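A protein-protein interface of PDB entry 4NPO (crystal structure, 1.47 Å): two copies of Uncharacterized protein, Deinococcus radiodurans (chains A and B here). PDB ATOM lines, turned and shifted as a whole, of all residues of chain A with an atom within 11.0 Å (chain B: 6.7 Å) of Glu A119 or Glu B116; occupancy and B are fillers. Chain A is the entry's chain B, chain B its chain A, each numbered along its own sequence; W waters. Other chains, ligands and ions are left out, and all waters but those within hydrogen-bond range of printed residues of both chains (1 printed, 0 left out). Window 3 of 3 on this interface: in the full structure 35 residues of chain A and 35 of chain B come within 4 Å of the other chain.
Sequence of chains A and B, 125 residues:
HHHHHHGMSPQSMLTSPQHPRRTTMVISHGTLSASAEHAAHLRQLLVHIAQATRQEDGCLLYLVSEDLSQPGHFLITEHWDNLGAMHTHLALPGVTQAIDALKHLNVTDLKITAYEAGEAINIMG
The backbone carbonyl oxygen (O) of Ala B114 sits at hydrogen-bond distance from the backbone NH (N) of Ile A121 (2.7 Å). The backbone carbonyl oxygen (O) of Glu B116 is in hydrogen-bond range of the backbone NH (N) of Gly A118, 2.7 Å away. N of Glu B116 is in hydrogen-bond range of O of Glu A119, 3.1 Å away. N of Gly B118 sits at hydrogen-bond distance from O of Glu A116, 2.8 Å away.
O of Ala B117 is in hydrogen-bond range of N of Thr B24 (2.5 Å). O of Met B25 is in hydrogen-bond range of N of Ala B117 (2.9 Å). The backbone carbonyl oxygen (O) of Ile B27 lies within hydrogen-bond range of the backbone NH (N) of Tyr B115, 2.7 Å away. The guanidinium group (NE) of Arg A21 is in salt-bridge range of the side-chain carboxylate (OE2) of Glu A119, at 2.7 Å. The backbone NH of Met A25 lies within hydrogen-bond range of the side-chain hydroxyl of Thr A23 (3.0 Å). The side-chain sulfur (SD) of Met A25 is in hydrogen-bond range of a ring nitrogen (ND1) of His A79 (3.7 Å).
Among the printed residues, merely in contact across the chains: Glu A119 with Tyr B115, Met A25 with Tyr B115, Tyr A115 with Gly B118, Ala A117 with Glu B116, Ile A27 with Tyr B115, Glu A116 with Ala B117, Ala A120 with Tyr B115, Ala A120 with Ala B114, Tyr A115 with Ile B27, Tyr A115 with Met B25, Glu A116 with Glu B116, Ala A117 with Tyr B115, His A79 with Tyr B115, Glu A119 with Ala B114, Tyr A115 with Ala B117 and Ile A123 with Ala B114.
Printed residues of chain B within 4 Å of Glu A119: Ala B114, Tyr B115 and Glu B116. Printed residues of chain A within 4 Å of Glu B116: Glu A116, Ala A117, Gly A118 and Glu A119. Printed residues of chain A within 4 Å of Ala B114: Glu A119, Ala A120, Ile A121 and Ile A123. Ala B117 touches two residues of chain A. Printed residues of chain B within 4 Å of His A79: Tyr B115. Of the printed residues of chain B, Met A25 touches Tyr B115. Of the printed residues of chain A, Tyr B115 touches Met A25 (3.4 Å), Ile A27 (3.5 Å), His A79 (3.9 Å), Ala A117 (3.8 Å), Glu A119 (3.1 Å) and Ala A120 (3.5 Å). The nearest printed residue of chain B that does not touch His A79 is Ile B27 (6.5 Å).
Of the 10 printed residues of chain B, 7 touch a printed residue of chain A. Printed residues of chain B that touch a printed residue of chain A: Met B25, Ile B27, Ala B114, Tyr B115, Glu B116, Ala B117 and Gly B118. Hydrophobic or aromatic side chains of chain B that line the printed part of chain A: Met B25, Ile B27, Ala B114, Tyr B115 and Ala B117. Of the 19 printed residues of chain A, 11 touch a printed residue of chain B. Hydrophobic or aromatic side chains of chain A that line the printed part of chain B: Met A25, Ile A27, His A79, Tyr A115, Ala A117, Ala A120, Ile A121 and Ile A123. Among the printed residues, 20 pairs touch across the chains. Among the printed residues, no Asp or Glu carboxylate lies within 4 Å of a Lys or Arg side-chain nitrogen of the other chain.
Met A25 touches Tyr B115, and with the chains exchanged Tyr A115 touches Met B25. Tyr A115 touches Gly B118, but with the chains exchanged Gly A118 does not touch Tyr B115 (5.4 Å). Glu A116 touches Ala B117, and with the chains exchanged Ala A117 touches Glu B116. Glu A116 touches Gly B118, and with the chains exchanged Gly A118 touches Glu B116. Positions printed for both chains: 24, 25, 26, 27, 114, 115, 116, 117 and 118.
Water W1 bridges the side-chain hydroxyl of Tyr B115 (2.6 Å) and the side-chain sulfur of Met A25 (3.8 Å).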
ATOM      1  N   ARG A  21     -20.966   0.120  30.050  1.00  0.00           N
ATOM      2  CA  ARG A  21     -21.660  -1.198  29.819  1.00  0.00           C
ATOM      3  C   ARG A  21     -22.352  -1.285  28.473  1.00  0.00           C
ATOM      4  O   ARG A  21     -22.746  -2.378  28.057  1.00  0.00           O
ATOM      5  CB  ARG A  21     -22.698  -1.512  30.909  1.00  0.00           C
ATOM      6  CG  ARG A  21     -22.149  -1.741  32.305  1.00  0.00           C
ATOM      7  CD  ARG A  21     -23.222  -2.308  33.231  1.00  0.00           C
ATOM      8  NE  ARG A  21     -24.309  -1.324  33.397  1.00  0.00           N
ATOM      9  CZ  ARG A  21     -24.187  -0.130  34.017  1.00  0.00           C
ATOM     10  NH1 ARG A  21     -23.033   0.222  34.535  1.00  0.00           N
ATOM     11  NH2 ARG A  21     -25.212   0.726  34.078  1.00  0.00           N
ATOM     12  N   ARG A  22     -22.521  -0.137  27.804  1.00  0.00           N
ATOM     13  CA  ARG A  22     -22.995  -0.129  26.419  1.00  0.00           C
ATOM     14  C   ARG A  22     -21.981  -0.926  25.590  1.00  0.00           C
ATOM     15  O   ARG A  22     -20.768  -0.869  25.838  1.00  0.00           O
ATOM     16  CB  ARG A  22     -23.094   1.328  25.890  1.00  0.00           C
ATOM     17  N   THR A  23     -22.481  -1.698  24.625  1.00  0.00           N
ATOM     18  CA  THR A  23     -21.557  -2.481  23.823  1.00  0.00           C
ATOM     19  C   THR A  23     -22.146  -2.797  22.468  1.00  0.00           C
ATOM     20  O   THR A  23     -23.348  -2.821  22.317  1.00  0.00           O
ATOM     21  CB  THR A  23     -21.188  -3.799  24.536  1.00  0.00           C
ATOM     22  OG1 THR A  23     -20.135  -4.471  23.824  1.00  0.00           O
ATOM     23  CG2 THR A  23     -22.374  -4.721  24.691  1.00  0.00           C
ATOM     24  N   THR A  24     -21.259  -2.942  21.500  1.00  0.00           N
ATOM     25  CA  THR A  24     -21.634  -3.398  20.152  1.00  0.00           C
ATOM     26  C   THR A  24     -21.154  -4.825  19.995  1.00  0.00           C
ATOM     27  O   THR A  24     -21.296  -5.389  18.901  1.00  0.00           O
ATOM     28  CB  THR A  24     -21.009  -2.554  19.046  1.00  0.00           C
ATOM     29  OG1 THR A  24     -19.592  -2.513  19.182  1.00  0.00           O
ATOM     30  CG2 THR A  24     -21.519  -1.154  19.123  1.00  0.00           C
ATOM     31  N   MET A  25     -20.628  -5.436  21.065  1.00  0.00           N
ATOM     32  CA  MET A  25     -19.906  -6.688  20.932  1.00  0.00           C
ATOM     33  C   MET A  25     -20.848  -7.755  20.530  1.00  0.00           C
ATOM     34  O   MET A  25     -22.029  -7.729  20.907  1.00  0.00           O
ATOM     35  CB  MET A  25     -19.240  -7.074  22.238  1.00  0.00           C
ATOM     36  CG  MET A  25     -18.162  -8.109  22.143  1.00  0.00           C
ATOM     37  SD  MET A  25     -17.588  -8.731  23.753  1.00  0.00           S
ATOM     38  CE  MET A  25     -18.924  -9.849  24.055  1.00  0.00           C
ATOM     39  N   VAL A  26     -20.343  -8.696  19.752  1.00  0.00           N
ATOM     40  CA  VAL A  26     -21.086  -9.887  19.325  1.00  0.00           C
ATOM     41  C   VAL A  26     -20.434 -11.102  19.918  1.00  0.00           C
ATOM     42  O   VAL A  26     -19.207 -11.232  19.861  1.00  0.00           O
ATOM     43  CB  VAL A  26     -21.107  -9.991  17.808  1.00  0.00           C
ATOM     44  CG1 VAL A  26     -21.849 -11.209  17.355  1.00  0.00           C
ATOM     45  CG2 VAL A  26     -21.761  -8.766  17.252  1.00  0.00           C
ATOM     46  N   ILE A  27     -21.232 -12.001  20.427  1.00  0.00           N
ATOM     47  CA  ILE A  27     -20.745 -13.228  21.008  1.00  0.00           C
ATOM     48  C   ILE A  27     -21.121 -14.337  20.064  1.00  0.00           C
ATOM     49  O   ILE A  27     -22.258 -14.407  19.608  1.00  0.00           O
ATOM     50  CB  ILE A  27     -21.397 -13.465  22.376  1.00  0.00           C
ATOM     51  CG1 ILE A  27     -20.911 -12.430  23.334  1.00  0.00           C
ATOM     52  CG2 ILE A  27     -21.130 -14.906  22.843  1.00  0.00           C
ATOM     53  CD1 ILE A  27     -21.628 -12.427  24.694  1.00  0.00           C
ATOM     54  N   HIS A  79     -15.650 -13.497  20.547  1.00  0.00           N
ATOM     55  CA  HIS A  79     -16.168 -12.153  20.778  1.00  0.00           C
ATOM     56  C   HIS A  79     -15.663 -11.286  19.645  1.00  0.00           C
ATOM     57  O   HIS A  79     -14.475 -11.292  19.387  1.00  0.00           O
ATOM     58  CB  HIS A  79     -15.711 -11.522  22.106  1.00  0.00           C
ATOM     59  CG  HIS A  79     -16.151 -12.254  23.311  1.00  0.00           C
ATOM     60  ND1 HIS A  79     -15.767 -11.859  24.566  1.00  0.00           N
ATOM     61  CD2 HIS A  79     -17.042 -13.265  23.481  1.00  0.00           C
ATOM     62  CE1 HIS A  79     -16.328 -12.641  25.461  1.00  0.00           C
ATOM     63  NE2 HIS A  79     -17.102 -13.501  24.831  1.00  0.00           N
ATOM     64  N   ASP A  81     -15.917  -7.349  17.813  1.00  0.00           N
ATOM     65  CA  ASP A  81     -16.130  -5.984  18.199  1.00  0.00           C
ATOM     66  C   ASP A  81     -17.533  -5.523  17.907  1.00  0.00           C
ATOM     67  O   ASP A  81     -18.116  -4.740  18.629  1.00  0.00           O
ATOM     68  CB  ASP A  81     -15.275  -5.092  17.304  1.00  0.00           C
ATOM     69  CG  ASP A  81     -14.948  -3.792  17.958  1.00  0.00           C
ATOM     70  OD1 ASP A  81     -15.000  -3.690  19.195  1.00  0.00           O
ATOM     71  OD2 ASP A  81     -14.785  -2.846  17.164  1.00  0.00           O
ATOM     72  N   ALA A 114     -24.721 -16.954  17.154  1.00  0.00           N
ATOM     73  CA  ALA A 114     -24.161 -15.694  17.608  1.00  0.00           C
ATOM     74  C   ALA A 114     -25.266 -14.791  18.092  1.00  0.00           C
ATOM     75  O   ALA A 114     -26.455 -15.028  17.853  1.00  0.00           O
ATOM     76  CB  ALA A 114     -23.401 -15.024  16.466  1.00  0.00           C
ATOM     77  N   TYR A 115     -24.871 -13.797  18.881  1.00  0.00           N
ATOM     78  CA  TYR A 115     -25.788 -12.902  19.536  1.00  0.00           C
ATOM     79  C   TYR A 115     -25.159 -11.548  19.645  1.00  0.00           C
ATOM     80  O   TYR A 115     -24.011 -11.429  20.107  1.00  0.00           O
ATOM     81  CB  TYR A 115     -26.081 -13.367  20.956  1.00  0.00           C
ATOM     82  CG  TYR A 115     -26.543 -14.782  21.103  1.00  0.00           C
ATOM     83  CD1 TYR A 115     -25.624 -15.802  21.186  1.00  0.00           C
ATOM     84  CD2 TYR A 115     -27.875 -15.111  21.179  1.00  0.00           C
ATOM     85  CE1 TYR A 115     -25.993 -17.107  21.329  1.00  0.00           C
ATOM     86  CE2 TYR A 115     -28.267 -16.426  21.310  1.00  0.00           C
ATOM     87  CZ  TYR A 115     -27.321 -17.420  21.385  1.00  0.00           C
ATOM     88  OH  TYR A 115     -27.752 -18.734  21.521  1.00  0.00           O
ATOM     89  N   GLU A 116     -25.917 -10.491  19.380  1.00  0.00           N
ATOM     90  CA  GLU A 116     -25.474  -9.203  19.700  1.00  0.00           C
ATOM     91  C   GLU A 116     -25.578  -9.051  21.162  1.00  0.00           C
ATOM     92  O   GLU A 116     -26.600  -9.415  21.730  1.00  0.00           O
ATOM     93  CB  GLU A 116     -26.355  -8.140  19.008  1.00  0.00           C
ATOM     94  CG  GLU A 116     -25.380  -7.086  18.506  1.00  0.00           C
ATOM     95  CD  GLU A 116     -26.059  -5.858  18.045  1.00  0.00           C
ATOM     96  OE1 GLU A 116     -27.251  -5.998  17.631  1.00  0.00           O
ATOM     97  OE2 GLU A 116     -25.375  -4.809  18.109  1.00  0.00           O
ATOM     98  N   ALA A 117     -24.558  -8.558  21.810  1.00  0.00           N
ATOM     99  CA  ALA A 117     -24.588  -8.314  23.252  1.00  0.00           C
ATOM    100  C   ALA A 117     -25.008  -6.844  23.437  1.00  0.00           C
ATOM    101  O   ALA A 117     -24.539  -5.984  22.722  1.00  0.00           O
ATOM    102  CB  ALA A 117     -23.229  -8.615  23.821  1.00  0.00           C
ATOM    103  N   GLY A 118     -26.032  -6.602  24.265  1.00  0.00           N
ATOM    104  CA  GLY A 118     -26.720  -5.291  24.351  1.00  0.00           C
ATOM    105  C   GLY A 118     -26.157  -4.508  25.520  1.00  0.00           C
ATOM    106  O   GLY A 118     -26.257  -3.256  25.612  1.00  0.00           O
ATOM    107  N   GLU A 119     -25.569  -5.251  26.439  1.00  0.00           N
ATOM    108  CA  GLU A 119     -24.956  -4.633  27.596  1.00  0.00           C
ATOM    109  C   GLU A 119     -23.946  -5.649  28.088  1.00  0.00           C
ATOM    110  O   GLU A 119     -24.247  -6.837  27.975  1.00  0.00           O
ATOM    111  CB  GLU A 119     -25.994  -4.441  28.692  1.00  0.00           C
ATOM    112  CG  GLU A 119     -25.488  -3.521  29.788  1.00  0.00           C
ATOM    113  CD  GLU A 119     -26.456  -3.376  30.936  1.00  0.00           C
ATOM    114  OE1 GLU A 119     -27.622  -3.807  30.808  1.00  0.00           O
ATOM    115  OE2 GLU A 119     -26.025  -2.857  31.976  1.00  0.00           O
ATOM    116  N   ALA A 120     -22.802  -5.163  28.550  1.00  0.00           N
ATOM    117  CA  ALA A 120     -21.692  -5.901  29.147  1.00  0.00           C
ATOM    118  C   ALA A 120     -21.511  -5.553  30.640  1.00  0.00           C
ATOM    119  O   ALA A 120     -21.264  -4.395  31.036  1.00  0.00           O
ATOM    120  CB  ALA A 120     -20.420  -5.548  28.402  1.00  0.00           C
ATOM    121  N   ILE A 121     -21.657  -6.548  31.466  1.00  0.00           N
ATOM    122  CA  ILE A 121     -21.894  -6.368  32.884  1.00  0.00           C
ATOM    123  C   ILE A 121     -20.802  -7.111  33.602  1.00  0.00           C
ATOM    124  O   ILE A 121     -20.770  -8.358  33.572  1.00  0.00           O
ATOM    125  CB  ILE A 121     -23.244  -6.890  33.307  1.00  0.00           C
ATOM    126  CG1 ILE A 121     -24.358  -6.242  32.524  1.00  0.00           C
ATOM    127  CG2 ILE A 121     -23.481  -6.785  34.802  1.00  0.00           C
ATOM    128  CD1 ILE A 121     -25.674  -6.983  32.641  1.00  0.00           C
ATOM    129  N   ASN A 122     -19.946  -6.405  34.317  1.00  0.00           N
ATOM    130  CA  ASN A 122     -18.930  -7.063  35.110  1.00  0.00           C
ATOM    131  C   ASN A 122     -19.540  -7.699  36.305  1.00  0.00           C
ATOM    132  O   ASN A 122     -20.226  -7.002  37.039  1.00  0.00           O
ATOM    133  CB  ASN A 122     -17.762  -6.231  35.568  1.00  0.00           C
ATOM    134  CG  ASN A 122     -16.797  -7.081  36.394  1.00  0.00           C
ATOM    135  OD1 ASN A 122     -16.887  -7.094  37.609  1.00  0.00           O
ATOM    136  ND2 ASN A 122     -16.043  -7.970  35.737  1.00  0.00           N
ATOM    137  N   ILE A 123     -19.347  -8.985  36.526  1.00  0.00           N
ATOM    138  CA  ILE A 123     -19.891  -9.710  37.649  1.00  0.00           C
ATOM    139  C   ILE A 123     -18.825  -9.804  38.688  1.00  0.00           C
ATOM    140  O   ILE A 123     -19.070  -9.483  39.849  1.00  0.00           O
ATOM    141  CB  ILE A 123     -20.398 -11.109  37.235  1.00  0.00           C
ATOM    142  CG1 ILE A 123     -21.506 -10.997  36.228  1.00  0.00           C
ATOM    143  CG2 ILE A 123     -20.795 -11.901  38.465  1.00  0.00           C
ATOM    144  CD1 ILE A 123     -22.716 -10.211  36.675  1.00  0.00           C
ATOM    145  N   THR B  24     -32.667 -11.980  24.543  1.00  0.00           N
ATOM    146  CA  THR B  24     -33.383 -13.268  24.602  1.00  0.00           C
ATOM    147  C   THR B  24     -33.080 -14.018  25.885  1.00  0.00           C
ATOM    148  O   THR B  24     -33.736 -15.018  26.197  1.00  0.00           O
ATOM    149  CB  THR B  24     -33.062 -14.174  23.354  1.00  0.00           C
ATOM    150  OG1 THR B  24     -31.614 -14.390  23.100  1.00  0.00           O
ATOM    151  CG2 THR B  24     -33.745 -13.563  22.173  1.00  0.00           C
ATOM    152  N   MET B  25     -32.111 -13.516  26.651  1.00  0.00           N
ATOM    153  CA  MET B  25     -31.275 -14.404  27.429  1.00  0.00           C
ATOM    154  C   MET B  25     -30.023 -13.641  27.882  1.00  0.00           C
ATOM    155  O   MET B  25     -29.687 -12.629  27.278  1.00  0.00           O
ATOM    156  CB  MET B  25     -30.854 -15.456  26.416  1.00  0.00           C
ATOM    157  CG  MET B  25     -30.068 -16.588  26.904  1.00  0.00           C
ATOM    158  SD  MET B  25     -29.661 -17.851  25.699  1.00  0.00           S
ATOM    159  CE  MET B  25     -28.402 -16.916  24.876  1.00  0.00           C
ATOM    160  N   VAL B  26     -29.378 -14.125  28.926  1.00  0.00           N
ATOM    161  CA  VAL B  26     -28.138 -13.580  29.419  1.00  0.00           C
ATOM    162  C   VAL B  26     -27.025 -14.596  29.238  1.00  0.00           C
ATOM    163  O   VAL B  26     -27.221 -15.781  29.509  1.00  0.00           O
ATOM    164  CB  VAL B  26     -28.237 -13.194  30.904  1.00  0.00           C
ATOM    165  CG1 VAL B  26     -26.867 -12.807  31.440  1.00  0.00           C
ATOM    166  CG2 VAL B  26     -29.192 -12.027  31.014  1.00  0.00           C
ATOM    167  N   ILE B  27     -25.927 -14.118  28.660  1.00  0.00           N
ATOM    168  CA  ILE B  27     -24.778 -14.946  28.472  1.00  0.00           C
ATOM    169  C   ILE B  27     -23.717 -14.553  29.440  1.00  0.00           C
ATOM    170  O   ILE B  27     -23.451 -13.367  29.609  1.00  0.00           O
ATOM    171  CB  ILE B  27     -24.219 -14.780  27.065  1.00  0.00           C
ATOM    172  CG1 ILE B  27     -25.197 -15.338  26.107  1.00  0.00           C
ATOM    173  CG2 ILE B  27     -22.864 -15.542  27.010  1.00  0.00           C
ATOM    174  CD1 ILE B  27     -24.939 -15.037  24.634  1.00  0.00           C
ATOM    175  N   LEU B  83     -31.629 -11.980  33.476  1.00  0.00           N
ATOM    176  CA  LEU B  83     -30.692 -11.495  34.436  1.00  0.00           C
ATOM    177  C   LEU B  83     -31.096 -11.888  35.839  1.00  0.00           C
ATOM    178  O   LEU B  83     -30.250 -12.178  36.691  1.00  0.00           O
ATOM    179  CB  LEU B  83     -30.502  -9.977  34.335  1.00  0.00           C
ATOM    180  CG  LEU B  83     -29.291  -9.462  35.070  1.00  0.00           C
ATOM    181  CD1 LEU B  83     -28.020  -9.990  34.456  1.00  0.00           C
ATOM    182  CD2 LEU B  83     -29.284  -7.932  35.011  1.00  0.00           C
ATOM    183  N   ALA B 114     -21.118 -10.740  32.188  1.00  0.00           N
ATOM    184  CA  ALA B 114     -22.408 -11.151  31.675  1.00  0.00           C
ATOM    185  C   ALA B 114     -22.889 -10.172  30.630  1.00  0.00           C
ATOM    186  O   ALA B 114     -22.475  -9.019  30.638  1.00  0.00           O
ATOM    187  CB  ALA B 114     -23.410 -11.241  32.786  1.00  0.00           C
ATOM    188  N   TYR B 115     -23.635 -10.669  29.673  1.00  0.00           N
ATOM    189  CA  TYR B 115     -24.120  -9.847  28.568  1.00  0.00           C
ATOM    190  C   TYR B 115     -25.574 -10.177  28.299  1.00  0.00           C
ATOM    191  O   TYR B 115     -26.013 -11.318  28.286  1.00  0.00           O
ATOM    192  CB  TYR B 115     -23.350 -10.197  27.306  1.00  0.00           C
ATOM    193  CG  TYR B 115     -21.859 -10.063  27.389  1.00  0.00           C
ATOM    194  CD1 TYR B 115     -21.116 -11.120  27.856  1.00  0.00           C
ATOM    195  CD2 TYR B 115     -21.212  -8.897  27.049  1.00  0.00           C
ATOM    196  CE1 TYR B 115     -19.742 -11.040  27.916  1.00  0.00           C
ATOM    197  CE2 TYR B 115     -19.846  -8.805  27.153  1.00  0.00           C
ATOM    198  CZ  TYR B 115     -19.147  -9.894  27.590  1.00  0.00           C
ATOM    199  OH  TYR B 115     -17.756  -9.808  27.662  1.00  0.00           O
ATOM    200  N   GLU B 116     -26.346  -9.124  28.180  1.00  0.00           N
ATOM    201  CA  GLU B 116     -27.704  -9.269  27.687  1.00  0.00           C
ATOM    202  C   GLU B 116     -27.687  -9.525  26.199  1.00  0.00           C
ATOM    203  O   GLU B 116     -27.176  -8.701  25.430  1.00  0.00           O
ATOM    204  CB  GLU B 116     -28.474  -7.980  27.968  1.00  0.00           C
ATOM    205  CG  GLU B 116     -28.749  -7.785  29.440  1.00  0.00           C
ATOM    206  CD  GLU B 116     -29.715  -6.648  29.661  1.00  0.00           C
ATOM    207  OE1 GLU B 116     -29.233  -5.560  29.965  1.00  0.00           O
ATOM    208  OE2 GLU B 116     -30.927  -6.841  29.486  1.00  0.00           O
ATOM    209  N   ALA B 117     -28.139 -10.685  25.813  1.00  0.00           N
ATOM    210  CA  ALA B 117     -28.029 -11.138  24.440  1.00  0.00           C
ATOM    211  C   ALA B 117     -29.275 -10.838  23.660  1.00  0.00           C
ATOM    212  O   ALA B 117     -30.392 -10.999  24.147  1.00  0.00           O
ATOM    213  CB  ALA B 117     -27.798 -12.625  24.423  1.00  0.00           C
ATOM    214  N   GLY B 118     -29.098 -10.421  22.437  1.00  0.00           N
ATOM    215  CA  GLY B 118     -30.218 -10.316  21.481  1.00  0.00           C
ATOM    216  C   GLY B 118     -30.613 -11.635  20.883  1.00  0.00           C
ATOM    217  O   GLY B 118     -30.277 -12.714  21.384  1.00  0.00           O
HETATM  218  O   HOH W   1     -16.674  -7.436  27.197  1.00  0.00           O
